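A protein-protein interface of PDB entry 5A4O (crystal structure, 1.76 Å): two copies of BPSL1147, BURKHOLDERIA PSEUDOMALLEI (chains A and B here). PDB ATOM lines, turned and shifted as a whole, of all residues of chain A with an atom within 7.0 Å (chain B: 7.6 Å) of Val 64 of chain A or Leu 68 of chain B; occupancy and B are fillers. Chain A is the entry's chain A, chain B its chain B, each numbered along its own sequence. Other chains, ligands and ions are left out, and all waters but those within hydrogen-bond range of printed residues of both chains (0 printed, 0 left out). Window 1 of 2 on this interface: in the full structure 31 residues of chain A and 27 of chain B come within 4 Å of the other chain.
Leu 70 of chain B touches Ile 10 of chain A. Ile 10 of chain A touches Glu 74 of chain B. Ile 23 of chain A touches Gly 67 of chain B (CD1 to CA, 3.9 Å). Ile 54 of chain A touches Val 36 of chain B. CG2 of Ile 56 of chain A touches CG1 of Ile 21 of chain B, 3.99 Å away. Leu 61 of chain A touches Leu 68 of chain B (CD2 to CD2, 3.9 Å). Val 64 of chain A touches Leu 68 of chain B. CG1 of Ile 65 of chain A touches CB of Leu 68 of chain B, at 3.7 Å. Gly 67 of chain A touches Ile 23 of chain B (CA to CD1, 3.6 Å). Leu 68 of chain A touches Val 36 of chain B (CD2 to CG2, 3.7 Å).
The backbone NH (N) of Val 34 of chain A lies within hydrogen-bond range of the backbone carbonyl oxygen (O) of Ile 56 of chain A. The backbone carbonyl oxygen (O) of Ala 11 of chain B is in hydrogen-bond range of the backbone NH (N) of Ile 23 of chain B (2.8 Å). N of Ile 10 of chain A sits at hydrogen-bond distance from O of Ile 23 of chain A. The backbone carbonyl oxygen of Val 36 of chain A lies within hydrogen-bond range of the backbone NH of Ile 54 of chain A (2.8 Å). The backbone carbonyl oxygen (O) of Val 13 of chain B is in hydrogen-bond range of the backbone NH (N) of Ile 21 of chain B, 2.8 Å away. The backbone carbonyl oxygen (O) of Leu 69 of chain B sits at hydrogen-bond distance from the side-chain hydroxyl (OG) of Ser 72 of chain B (2.4 Å).
Of chain B, only Ile 23 (3.6 Å) and Leu 68 (3.8 Å) come within 4 Å of Val 64 of chain A. Printed residues of chain A within 4 Å of Gly 67 of chain B: Ile 10 (3.5 Å), Ala 11 (3.9 Å) and Ile 23 (3.9 Å). Of the printed residues of chain A, Ile 65 of chain B touches Leu 68 and Leu 69. Of the printed residues of chain A, Leu 70 of chain B touches Ile 10. Of the printed residues of chain A, Glu 74 of chain B touches Ile 10 (3.7 Å). Printed residues of chain B within 4 Å of Ile 23 of chain A: Val 64 and Gly 67. Of the printed residues of chain B, Leu 61 of chain A touches Leu 68 (3.9 Å) and Ser 72 (3.8 Å). Gln 63 of chain B touches none of the printed residues of chain A. Leu 61 of chain B touches none of the printed residues of chain A. The nearest residue of chain B that does not touch Val 64 of chain A is Val 13 of chain B (4.1 Å).
Printed residues of chain B that touch a printed residue of chain A: Val 13, Ile 21, Ile 23, Val 36, Val 64, Ile 65, Gly 67, Leu 68, Leu 69, Leu 70, Ala 71, Ser 72 and Glu 74. Hydrophobic or aromatic side chains of chain B within 4 Å of the printed part of chain A: Val 13, Ile 21, Ile 23, Val 36, Ile 65, Leu 68, Leu 69 and Leu 70. Of the 19 printed residues of chain A, 13 touch a printed residue of chain B. Among the printed residues, 24 pairs touch across the chains. Among the printed residues, no Asp or Glu carboxylate lies within 4 Å of a Lys or Arg side-chain nitrogen of the other chain.
Ile 23 of chain A touches Val 64 of chain B, and with the chains exchanged Val 64 of chain A touches Ile 23 of chain B. Ile 23 of chain A touches Gly 67 of chain B, and with the chains exchanged Gly 67 of chain A touches Ile 23 of chain B. Leu 61 of chain A touches Leu 68 of chain B, but with the chains exchanged Leu 68 of chain A does not touch Leu 61 of chain B (4.03 Å). Leu 68 of chain A touches its own counterpart, Leu 68 of chain B. Positions printed for both chains: 11, 23, 36, 61, 62, 63, 64, 65, 66, 67, 68, 69 and 70. Of the 24 pairs that touch across the chains among the printed residues, 11 have their exchanged pair printed and touching as well.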
ATOM      1  N   ILE A  10       3.283 -12.286  22.912  1.00  0.00           N
ATOM      2  CA  ILE A  10       4.139 -13.108  23.771  1.00  0.00           C
ATOM      3  C   ILE A  10       5.524 -13.161  23.141  1.00  0.00           C
ATOM      4  O   ILE A  10       6.539 -13.006  23.830  1.00  0.00           O
ATOM      5  CB  ILE A  10       3.599 -14.550  23.894  1.00  0.00           C
ATOM      6  CG1 ILE A  10       2.147 -14.584  24.342  1.00  0.00           C
ATOM      7  CG2 ILE A  10       4.472 -15.381  24.828  1.00  0.00           C
ATOM      8  CD1 ILE A  10       1.855 -13.895  25.624  1.00  0.00           C
ATOM      9  N   ALA A  11       5.557 -13.387  21.829  1.00  0.00           N
ATOM     10  CA  ALA A  11       6.808 -13.444  21.063  1.00  0.00           C
ATOM     11  C   ALA A  11       6.673 -13.042  19.592  1.00  0.00           C
ATOM     12  O   ALA A  11       5.606 -13.166  18.928  1.00  0.00           O
ATOM     13  CB  ALA A  11       7.450 -14.823  21.179  1.00  0.00           C
ATOM     14  N   ILE A  23       3.412 -14.639  18.065  1.00  0.00           N
ATOM     15  CA  ILE A  23       2.740 -15.554  18.940  1.00  0.00           C
ATOM     16  C   ILE A  23       2.063 -14.643  19.922  1.00  0.00           C
ATOM     17  O   ILE A  23       2.738 -13.832  20.569  1.00  0.00           O
ATOM     18  CB  ILE A  23       3.743 -16.485  19.656  1.00  0.00           C
ATOM     19  CG1 ILE A  23       4.441 -17.387  18.607  1.00  0.00           C
ATOM     20  CG2 ILE A  23       3.034 -17.334  20.701  1.00  0.00           C
ATOM     21  CD1 ILE A  23       5.529 -18.252  19.173  1.00  0.00           C
ATOM     22  N   VAL A  34      -4.658 -18.950  21.814  1.00  0.00           N
ATOM     23  CA  VAL A  34      -3.260 -18.738  21.466  1.00  0.00           C
ATOM     24  C   VAL A  34      -3.179 -18.687  19.944  1.00  0.00           C
ATOM     25  O   VAL A  34      -3.690 -19.563  19.251  1.00  0.00           O
ATOM     26  CB  VAL A  34      -2.332 -19.840  22.009  1.00  0.00           C
ATOM     27  CG1 VAL A  34      -0.892 -19.634  21.534  1.00  0.00           C
ATOM     28  CG2 VAL A  34      -2.380 -19.853  23.530  1.00  0.00           C
ATOM     29  N   ASP A  35      -2.545 -17.647  19.427  1.00  0.00           N
ATOM     30  CA  ASP A  35      -2.474 -17.439  18.004  1.00  0.00           C
ATOM     31  C   ASP A  35      -1.015 -17.474  17.570  1.00  0.00           C
ATOM     32  O   ASP A  35      -0.143 -16.896  18.238  1.00  0.00           O
ATOM     33  CB  ASP A  35      -3.102 -16.083  17.718  1.00  0.00           C
ATOM     34  CG  ASP A  35      -3.451 -15.885  16.285  1.00  0.00           C
ATOM     35  OD1 ASP A  35      -4.487 -16.409  15.856  1.00  0.00           O
ATOM     36  OD2 ASP A  35      -2.711 -15.151  15.593  1.00  0.00           O
ATOM     37  N   VAL A  36      -0.742 -18.148  16.454  1.00  0.00           N
ATOM     38  CA  VAL A  36       0.609 -18.238  15.897  1.00  0.00           C
ATOM     39  C   VAL A  36       0.449 -17.875  14.442  1.00  0.00           C
ATOM     40  O   VAL A  36      -0.242 -18.575  13.725  1.00  0.00           O
ATOM     41  CB  VAL A  36       1.179 -19.659  16.012  1.00  0.00           C
ATOM     42  CG1 VAL A  36       2.548 -19.745  15.385  1.00  0.00           C
ATOM     43  CG2 VAL A  36       1.202 -20.098  17.471  1.00  0.00           C
ATOM     44  N   ILE A  54      -2.372 -20.221  12.850  1.00  0.00           N
ATOM     45  CA  ILE A  54      -3.281 -21.120  13.528  1.00  0.00           C
ATOM     46  C   ILE A  54      -3.793 -20.467  14.846  1.00  0.00           C
ATOM     47  O   ILE A  54      -3.129 -19.596  15.465  1.00  0.00           O
ATOM     48  CB  ILE A  54      -2.632 -22.504  13.775  1.00  0.00           C
ATOM     49  CG1 ILE A  54      -1.445 -22.367  14.705  1.00  0.00           C
ATOM     50  CG2 ILE A  54      -2.210 -23.176  12.475  1.00  0.00           C
ATOM     51  CD1 ILE A  54      -0.991 -23.653  15.337  1.00  0.00           C
ATOM     52  N   ILE A  56      -5.476 -21.788  18.507  1.00  0.00           N
ATOM     53  CA  ILE A  56      -5.735 -22.950  19.315  1.00  0.00           C
ATOM     54  C   ILE A  56      -6.093 -22.642  20.752  1.00  0.00           C
ATOM     55  O   ILE A  56      -5.691 -21.637  21.316  1.00  0.00           O
ATOM     56  CB  ILE A  56      -4.526 -23.876  19.340  1.00  0.00           C
ATOM     57  CG1 ILE A  56      -3.293 -23.143  19.861  1.00  0.00           C
ATOM     58  CG2 ILE A  56      -4.265 -24.419  17.942  1.00  0.00           C
ATOM     59  CD1 ILE A  56      -2.261 -24.089  20.341  1.00  0.00           C
ATOM     60  N   LEU A  60      -4.292 -27.564  23.994  1.00  0.00           N
ATOM     61  CA  LEU A  60      -3.512 -28.194  22.920  1.00  0.00           C
ATOM     62  C   LEU A  60      -2.041 -27.785  22.910  1.00  0.00           C
ATOM     63  O   LEU A  60      -1.249 -28.384  22.161  1.00  0.00           O
ATOM     64  CB  LEU A  60      -4.113 -27.859  21.541  1.00  0.00           C
ATOM     65  CG  LEU A  60      -5.512 -28.414  21.275  1.00  0.00           C
ATOM     66  CD1 LEU A  60      -5.901 -28.218  19.815  1.00  0.00           C
ATOM     67  CD2 LEU A  60      -5.633 -29.883  21.635  1.00  0.00           C
ATOM     68  N   LEU A  61      -1.661 -26.772  23.692  1.00  0.00           N
ATOM     69  CA  LEU A  61      -0.273 -26.290  23.711  1.00  0.00           C
ATOM     70  C   LEU A  61       0.799 -27.322  23.988  1.00  0.00           C
ATOM     71  O   LEU A  61       1.792 -27.374  23.278  1.00  0.00           O
ATOM     72  CB  LEU A  61      -0.089 -25.136  24.698  1.00  0.00           C
ATOM     73  CG  LEU A  61      -0.585 -23.803  24.208  1.00  0.00           C
ATOM     74  CD1 LEU A  61      -0.705 -22.855  25.401  1.00  0.00           C
ATOM     75  CD2 LEU A  61       0.331 -23.235  23.120  1.00  0.00           C
ATOM     76  N   ALA A  62       0.630 -28.128  25.019  1.00  0.00           N
ATOM     77  CA  ALA A  62       1.642 -29.136  25.362  1.00  0.00           C
ATOM     78  C   ALA A  62       1.880 -30.073  24.186  1.00  0.00           C
ATOM     79  O   ALA A  62       3.010 -30.380  23.855  1.00  0.00           O
ATOM     80  CB  ALA A  62       1.238 -29.945  26.601  1.00  0.00           C
ATOM     81  N   GLN A  63       0.803 -30.535  23.556  1.00  0.00           N
ATOM     82  CA  GLN A  63       0.950 -31.382  22.363  1.00  0.00           C
ATOM     83  C   GLN A  63       1.671 -30.697  21.208  1.00  0.00           C
ATOM     84  O   GLN A  63       2.522 -31.319  20.554  1.00  0.00           O
ATOM     85  CB  GLN A  63      -0.413 -31.914  21.922  1.00  0.00           C
ATOM     86  CG  GLN A  63      -1.010 -32.900  22.916  1.00  0.00           C
ATOM     87  CD  GLN A  63      -2.507 -33.039  22.756  1.00  0.00           C
ATOM     88  OE1 GLN A  63      -3.290 -32.386  23.442  1.00  0.00           O
ATOM     89  NE2 GLN A  63      -2.904 -33.840  21.787  1.00  0.00           N
ATOM     90  N   VAL A  64       1.326 -29.445  20.917  1.00  0.00           N
ATOM     91  CA  VAL A  64       1.993 -28.695  19.828  1.00  0.00           C
ATOM     92  C   VAL A  64       3.480 -28.506  20.138  1.00  0.00           C
ATOM     93  O   VAL A  64       4.330 -28.783  19.329  1.00  0.00           O
ATOM     94  CB  VAL A  64       1.289 -27.347  19.510  1.00  0.00           C
ATOM     95  CG1 VAL A  64       2.125 -26.474  18.581  1.00  0.00           C
ATOM     96  CG2 VAL A  64      -0.059 -27.601  18.876  1.00  0.00           C
ATOM     97  N   ILE A  65       3.778 -28.085  21.355  1.00  0.00           N
ATOM     98  CA  ILE A  65       5.163 -27.953  21.799  1.00  0.00           C
ATOM     99  C   ILE A  65       5.930 -29.265  21.641  1.00  0.00           C
ATOM    100  O   ILE A  65       7.059 -29.297  21.129  1.00  0.00           O
ATOM    101  CB  ILE A  65       5.216 -27.469  23.242  1.00  0.00           C
ATOM    102  CG1 ILE A  65       4.857 -25.992  23.311  1.00  0.00           C
ATOM    103  CG2 ILE A  65       6.605 -27.701  23.825  1.00  0.00           C
ATOM    104  CD1 ILE A  65       4.392 -25.480  24.674  1.00  0.00           C
ATOM    105  N   GLN A  66       5.325 -30.359  22.094  1.00  0.00           N
ATOM    106  CA  GLN A  66       5.983 -31.646  21.999  1.00  0.00           C
ATOM    107  C   GLN A  66       6.199 -32.066  20.555  1.00  0.00           C
ATOM    108  O   GLN A  66       7.231 -32.608  20.227  1.00  0.00           O
ATOM    109  CB  GLN A  66       5.222 -32.719  22.764  1.00  0.00           C
ATOM    110  CG  GLN A  66       5.477 -32.718  24.287  1.00  0.00           C
ATOM    111  CD  GLN A  66       6.875 -32.332  24.758  1.00  0.00           C
ATOM    112  OE1 GLN A  66       7.041 -31.392  25.560  1.00  0.00           O
ATOM    113  NE2 GLN A  66       7.889 -33.064  24.299  1.00  0.00           N
ATOM    114  N   GLY A  67       5.230 -31.785  19.675  1.00  0.00           N
ATOM    115  CA  GLY A  67       5.431 -32.022  18.250  1.00  0.00           C
ATOM    116  C   GLY A  67       6.571 -31.227  17.621  1.00  0.00           C
ATOM    117  O   GLY A  67       7.345 -31.748  16.803  1.00  0.00           O
ATOM    118  N   LEU A  68       6.711 -29.969  18.024  1.00  0.00           N
ATOM    119  CA  LEU A  68       7.762 -29.125  17.485  1.00  0.00           C
ATOM    120  C   LEU A  68       9.123 -29.529  18.025  1.00  0.00           C
ATOM    121  O   LEU A  68      10.111 -29.495  17.288  1.00  0.00           O
ATOM    122  CB  LEU A  68       7.510 -27.647  17.798  1.00  0.00           C
ATOM    123  CG  LEU A  68       6.245 -27.035  17.179  1.00  0.00           C
ATOM    124  CD1 LEU A  68       6.003 -25.690  17.826  1.00  0.00           C
ATOM    125  CD2 LEU A  68       6.337 -26.900  15.671  1.00  0.00           C
ATOM    126  N   LEU A  69       9.167 -29.961  19.276  1.00  0.00           N
ATOM    127  CA  LEU A  69      10.410 -30.483  19.856  1.00  0.00           C
ATOM    128  C   LEU A  69      10.856 -31.718  19.074  1.00  0.00           C
ATOM    129  O   LEU A  69      12.019 -31.858  18.728  1.00  0.00           O
ATOM    130  CB  LEU A  69      10.223 -30.823  21.339  1.00  0.00           C
ATOM    131  CG  LEU A  69      10.176 -29.651  22.295  1.00  0.00           C
ATOM    132  CD1 LEU A  69       9.756 -30.124  23.674  1.00  0.00           C
ATOM    133  CD2 LEU A  69      11.563 -29.018  22.362  1.00  0.00           C
ATOM    134  N   LEU A  70       9.913 -32.612  18.799  1.00  0.00           N
ATOM    135  CA  LEU A  70      10.194 -33.800  17.992  1.00  0.00           C
ATOM    136  C   LEU A  70      10.712 -33.424  16.605  1.00  0.00           C
ATOM    137  O   LEU A  70      11.660 -34.038  16.123  1.00  0.00           O
ATOM    138  CB  LEU A  70       8.938 -34.658  17.861  1.00  0.00           C
ATOM    139  CG  LEU A  70       9.066 -36.042  17.251  1.00  0.00           C
ATOM    140  CD1 LEU A  70      10.131 -36.815  18.012  1.00  0.00           C
ATOM    141  CD2 LEU A  70       7.757 -36.795  17.338  1.00  0.00           C
ATOM    142  N   ALA B  11       3.741 -34.903  13.575  1.00  0.00           N
ATOM    143  CA  ALA B  11       2.710 -35.068  14.608  1.00  0.00           C
ATOM    144  C   ALA B  11       1.407 -34.420  14.137  1.00  0.00           C
ATOM    145  O   ALA B  11       1.430 -33.402  13.466  1.00  0.00           O
ATOM    146  CB  ALA B  11       3.161 -34.411  15.901  1.00  0.00           C
ATOM    147  N   VAL B  13      -1.965 -33.032  15.832  1.00  0.00           N
ATOM    148  CA  VAL B  13      -2.643 -32.647  17.063  1.00  0.00           C
ATOM    149  C   VAL B  13      -4.125 -32.461  16.788  1.00  0.00           C
ATOM    150  O   VAL B  13      -4.505 -31.604  15.986  1.00  0.00           O
ATOM    151  CB  VAL B  13      -2.031 -31.366  17.652  1.00  0.00           C
ATOM    152  CG1 VAL B  13      -2.764 -30.934  18.922  1.00  0.00           C
ATOM    153  CG2 VAL B  13      -0.553 -31.576  17.882  1.00  0.00           C
ATOM    154  N   ILE B  21      -4.175 -29.866  13.858  1.00  0.00           N
ATOM    155  CA  ILE B  21      -2.963 -29.102  13.595  1.00  0.00           C
ATOM    156  C   ILE B  21      -1.842 -30.121  13.266  1.00  0.00           C
ATOM    157  O   ILE B  21      -1.392 -30.897  14.144  1.00  0.00           O
ATOM    158  CB  ILE B  21      -2.515 -28.269  14.826  1.00  0.00           C
ATOM    159  CG1 ILE B  21      -3.617 -27.326  15.281  1.00  0.00           C
ATOM    160  CG2 ILE B  21      -1.245 -27.453  14.532  1.00  0.00           C
ATOM    161  CD1 ILE B  21      -4.185 -26.479  14.170  1.00  0.00           C
ATOM    162  N   ARG B  22      -1.404 -30.102  12.019  1.00  0.00           N
ATOM    163  CA  ARG B  22      -0.382 -31.004  11.524  1.00  0.00           C
ATOM    164  C   ARG B  22       0.974 -30.323  11.479  1.00  0.00           C
ATOM    165  O   ARG B  22       1.118 -29.233  10.936  1.00  0.00           O
ATOM    166  CB  ARG B  22      -0.738 -31.541  10.145  1.00  0.00           C
ATOM    167  CG  ARG B  22       0.312 -32.516   9.586  1.00  0.00           C
ATOM    168  CD  ARG B  22      -0.234 -33.157   8.351  1.00  0.00           C
ATOM    169  NE  ARG B  22      -1.296 -34.063   8.763  1.00  0.00           N
ATOM    170  CZ  ARG B  22      -2.113 -34.712   7.941  1.00  0.00           C
ATOM    171  NH1 ARG B  22      -2.038 -34.522   6.640  1.00  0.00           N
ATOM    172  NH2 ARG B  22      -2.998 -35.561   8.448  1.00  0.00           N
ATOM    173  N   ILE B  23       1.955 -30.980  12.090  1.00  0.00           N
ATOM    174  CA  ILE B  23       3.328 -30.507  12.112  1.00  0.00           C
ATOM    175  C   ILE B  23       4.068 -31.447  11.176  1.00  0.00           C
ATOM    176  O   ILE B  23       4.029 -32.649  11.354  1.00  0.00           O
ATOM    177  CB  ILE B  23       3.946 -30.619  13.518  1.00  0.00           C
ATOM    178  CG1 ILE B  23       3.225 -29.662  14.492  1.00  0.00           C
ATOM    179  CG2 ILE B  23       5.428 -30.263  13.512  1.00  0.00           C
ATOM    180  CD1 ILE B  23       3.573 -29.888  15.952  1.00  0.00           C
ATOM    181  N   VAL B  36       3.463 -25.985  10.001  1.00  0.00           N
ATOM    182  CA  VAL B  36       2.479 -26.103  11.046  1.00  0.00           C
ATOM    183  C   VAL B  36       1.171 -25.538  10.469  1.00  0.00           C
ATOM    184  O   VAL B  36       1.104 -24.376  10.130  1.00  0.00           O
ATOM    185  CB  VAL B  36       2.870 -25.308  12.317  1.00  0.00           C
ATOM    186  CG1 VAL B  36       1.791 -25.485  13.360  1.00  0.00           C
ATOM    187  CG2 VAL B  36       4.248 -25.752  12.826  1.00  0.00           C
ATOM    188  N   LEU B  61      12.866 -22.599  14.866  1.00  0.00           N
ATOM    189  CA  LEU B  61      12.073 -23.459  15.695  1.00  0.00           C
ATOM    190  C   LEU B  61      12.212 -23.195  17.186  1.00  0.00           C
ATOM    191  O   LEU B  61      11.203 -23.172  17.881  1.00  0.00           O
ATOM    192  CB  LEU B  61      12.356 -24.963  15.473  1.00  0.00           C
ATOM    193  CG  LEU B  61      11.592 -25.741  14.425  1.00  0.00           C
ATOM    194  CD1 LEU B  61      12.217 -27.126  14.247  1.00  0.00           C
ATOM    195  CD2 LEU B  61      10.128 -25.872  14.763  1.00  0.00           C
ATOM    196  N   ALA B  62      13.450 -23.071  17.686  1.00  0.00           N
ATOM    197  CA  ALA B  62      13.646 -22.836  19.124  1.00  0.00           C
ATOM    198  C   ALA B  62      12.858 -21.614  19.635  1.00  0.00           C
ATOM    199  O   ALA B  62      12.254 -21.660  20.692  1.00  0.00           O
ATOM    200  CB  ALA B  62      15.128 -22.712  19.455  1.00  0.00           C
ATOM    201  N   GLN B  63      12.842 -20.539  18.867  1.00  0.00           N
ATOM    202  CA  GLN B  63      12.165 -19.346  19.242  1.00  0.00           C
ATOM    203  C   GLN B  63      10.656 -19.549  19.245  1.00  0.00           C
ATOM    204  O   GLN B  63       9.945 -19.008  20.096  1.00  0.00           O
ATOM    205  CB  GLN B  63      12.562 -18.255  18.273  1.00  0.00           C
ATOM    206  CG  GLN B  63      13.876 -17.588  18.649  1.00  0.00           C
ATOM    207  CD  GLN B  63      14.390 -16.725  17.509  1.00  0.00           C
ATOM    208  OE1 GLN B  63      15.186 -17.163  16.715  1.00  0.00           O
ATOM    209  NE2 GLN B  63      13.875 -15.540  17.401  1.00  0.00           N
ATOM    210  N   VAL B  64      10.161 -20.328  18.281  1.00  0.00           N
ATOM    211  CA  VAL B  64       8.739 -20.595  18.239  1.00  0.00           C
ATOM    212  C   VAL B  64       8.348 -21.457  19.442  1.00  0.00           C
ATOM    213  O   VAL B  64       7.347 -21.207  20.100  1.00  0.00           O
ATOM    214  CB  VAL B  64       8.327 -21.228  16.907  1.00  0.00           C
ATOM    215  CG1 VAL B  64       6.874 -21.684  16.942  1.00  0.00           C
ATOM    216  CG2 VAL B  64       8.538 -20.212  15.798  1.00  0.00           C
ATOM    217  N   ILE B  65       9.151 -22.467  19.733  1.00  0.00           N
ATOM    218  CA  ILE B  65       8.955 -23.306  20.939  1.00  0.00           C
ATOM    219  C   ILE B  65       8.935 -22.456  22.210  1.00  0.00           C
ATOM    220  O   ILE B  65       8.037 -22.605  23.046  1.00  0.00           O
ATOM    221  CB  ILE B  65      10.024 -24.442  21.043  1.00  0.00           C
ATOM    222  CG1 ILE B  65       9.819 -25.452  19.915  1.00  0.00           C
ATOM    223  CG2 ILE B  65       9.911 -25.186  22.366  1.00  0.00           C
ATOM    224  CD1 ILE B  65      10.951 -26.385  19.627  1.00  0.00           C
ATOM    225  N   GLN B  66       9.947 -21.616  22.372  1.00  0.00           N
ATOM    226  CA  GLN B  66      10.039 -20.770  23.569  1.00  0.00           C
ATOM    227  C   GLN B  66       8.857 -19.825  23.709  1.00  0.00           C
ATOM    228  O   GLN B  66       8.358 -19.609  24.810  1.00  0.00           O
ATOM    229  CB  GLN B  66      11.396 -20.064  23.613  1.00  0.00           C
ATOM    230  CG  GLN B  66      12.488 -21.092  23.866  1.00  0.00           C
ATOM    231  CD  GLN B  66      13.851 -20.515  24.130  1.00  0.00           C
ATOM    232  OE1 GLN B  66      14.095 -19.323  23.931  1.00  0.00           O
ATOM    233  NE2 GLN B  66      14.771 -21.381  24.560  1.00  0.00           N
ATOM    234  N   GLY B  67       8.372 -19.276  22.596  1.00  0.00           N
ATOM    235  CA  GLY B  67       7.194 -18.454  22.656  1.00  0.00           C
ATOM    236  C   GLY B  67       5.948 -19.195  23.116  1.00  0.00           C
ATOM    237  O   GLY B  67       5.141 -18.648  23.858  1.00  0.00           O
ATOM    238  N   LEU B  68       5.790 -20.431  22.658  1.00  0.00           N
ATOM    239  CA  LEU B  68       4.663 -21.253  23.066  1.00  0.00           C
ATOM    240  C   LEU B  68       4.756 -21.651  24.536  1.00  0.00           C
ATOM    241  O   LEU B  68       3.730 -21.713  25.202  1.00  0.00           O
ATOM    242  CB  LEU B  68       4.532 -22.481  22.156  1.00  0.00           C
ATOM    243  CG  LEU B  68       4.142 -22.213  20.709  1.00  0.00           C
ATOM    244  CD1 LEU B  68       4.075 -23.516  19.933  1.00  0.00           C
ATOM    245  CD2 LEU B  68       2.783 -21.532  20.645  1.00  0.00           C
ATOM    246  N   LEU B  69       5.966 -21.965  25.008  1.00  0.00           N
ATOM    247  CA  LEU B  69       6.187 -22.234  26.416  1.00  0.00           C
ATOM    248  C   LEU B  69       5.760 -21.054  27.264  1.00  0.00           C
ATOM    249  O   LEU B  69       5.078 -21.245  28.251  1.00  0.00           O
ATOM    250  CB  LEU B  69       7.651 -22.584  26.684  1.00  0.00           C
ATOM    251  CG  LEU B  69       8.029 -23.983  26.216  1.00  0.00           C
ATOM    252  CD1 LEU B  69       9.542 -24.137  26.206  1.00  0.00           C
ATOM    253  CD2 LEU B  69       7.385 -25.080  27.070  1.00  0.00           C
ATOM    254  N   LEU B  70       6.122 -19.841  26.861  1.00  0.00           N
ATOM    255  CA  LEU B  70       5.655 -18.628  27.538  1.00  0.00           C
ATOM    256  C   LEU B  70       4.162 -18.405  27.471  1.00  0.00           C
ATOM    257  O   LEU B  70       3.505 -18.005  28.477  1.00  0.00           O
ATOM    258  CB  LEU B  70       6.360 -17.396  26.961  1.00  0.00           C
ATOM    259  CG  LEU B  70       7.801 -17.223  27.357  1.00  0.00           C
ATOM    260  CD1 LEU B  70       8.313 -15.909  26.755  1.00  0.00           C
ATOM    261  CD2 LEU B  70       7.914 -17.158  28.874  1.00  0.00           C
ATOM    262  N   ALA B  71       3.568 -18.690  26.312  1.00  0.00           N
ATOM    263  CA  ALA B  71       2.147 -18.494  26.143  1.00  0.00           C
ATOM    264  C   ALA B  71       1.377 -19.449  27.073  1.00  0.00           C
ATOM    265  O   ALA B  71       0.251 -19.159  27.474  1.00  0.00           O
ATOM    266  CB  ALA B  71       1.749 -18.702  24.683  1.00  0.00           C
ATOM    267  N   SER B  72       1.992 -20.580  27.419  1.00  0.00           N
ATOM    268  CA  SER B  72       1.361 -21.560  28.293  1.00  0.00           C
ATOM    269  C   SER B  72       1.167 -21.021  29.722  1.00  0.00           C
ATOM    270  O   SER B  72       0.338 -21.522  30.450  1.00  0.00           O
ATOM    271  CB  SER B  72       2.188 -22.848  28.333  1.00  0.00           C
ATOM    272  OG  SER B  72       3.354 -22.699  29.139  1.00  0.00           O
ATOM    273  N   ARG B  73       1.965 -20.031  30.104  1.00  0.00           N
ATOM    274  CA  ARG B  73       1.859 -19.376  31.448  1.00  0.00           C
ATOM    275  C   ARG B  73       0.737 -18.382  31.592  1.00  0.00           C
ATOM    276  O   ARG B  73       0.421 -17.966  32.709  1.00  0.00           O
ATOM    277  CB  ARG B  73       3.143 -18.639  31.786  1.00  0.00           C
ATOM    278  CG  ARG B  73       4.362 -19.507  31.871  1.00  0.00           C
ATOM    279  CD  ARG B  73       5.550 -18.643  32.243  1.00  0.00           C
ATOM    280  NE  ARG B  73       6.761 -19.430  32.318  1.00  0.00           N
ATOM    281  CZ  ARG B  73       8.006 -18.946  32.369  1.00  0.00           C
ATOM    282  NH1 ARG B  73       8.262 -17.640  32.356  1.00  0.00           N
ATOM    283  NH2 ARG B  73       9.006 -19.811  32.408  1.00  0.00           N
ATOM    284  N   GLU B  74       0.156 -17.953  30.479  1.00  0.00           N
ATOM    285  CA  GLU B  74      -1.002 -17.093  30.532  1.00  0.00           C
ATOM    286  C   GLU B  74      -2.096 -18.025  31.038  1.00  0.00           C
ATOM    287  O   GLU B  74      -1.936 -19.235  31.047  1.00  0.00           O
ATOM    288  CB  GLU B  74      -1.310 -16.524  29.159  1.00  0.00           C
ATOM    289  CG  GLU B  74      -0.154 -15.752  28.553  1.00  0.00           C
ATOM    290  CD  GLU B  74       0.155 -14.448  29.283  1.00  0.00           C
ATOM    291  OE1 GLU B  74      -0.773 -13.809  29.814  1.00  0.00           O
ATOM    292  OE2 GLU B  74       1.321 -14.017  29.270  1.00  0.00           O
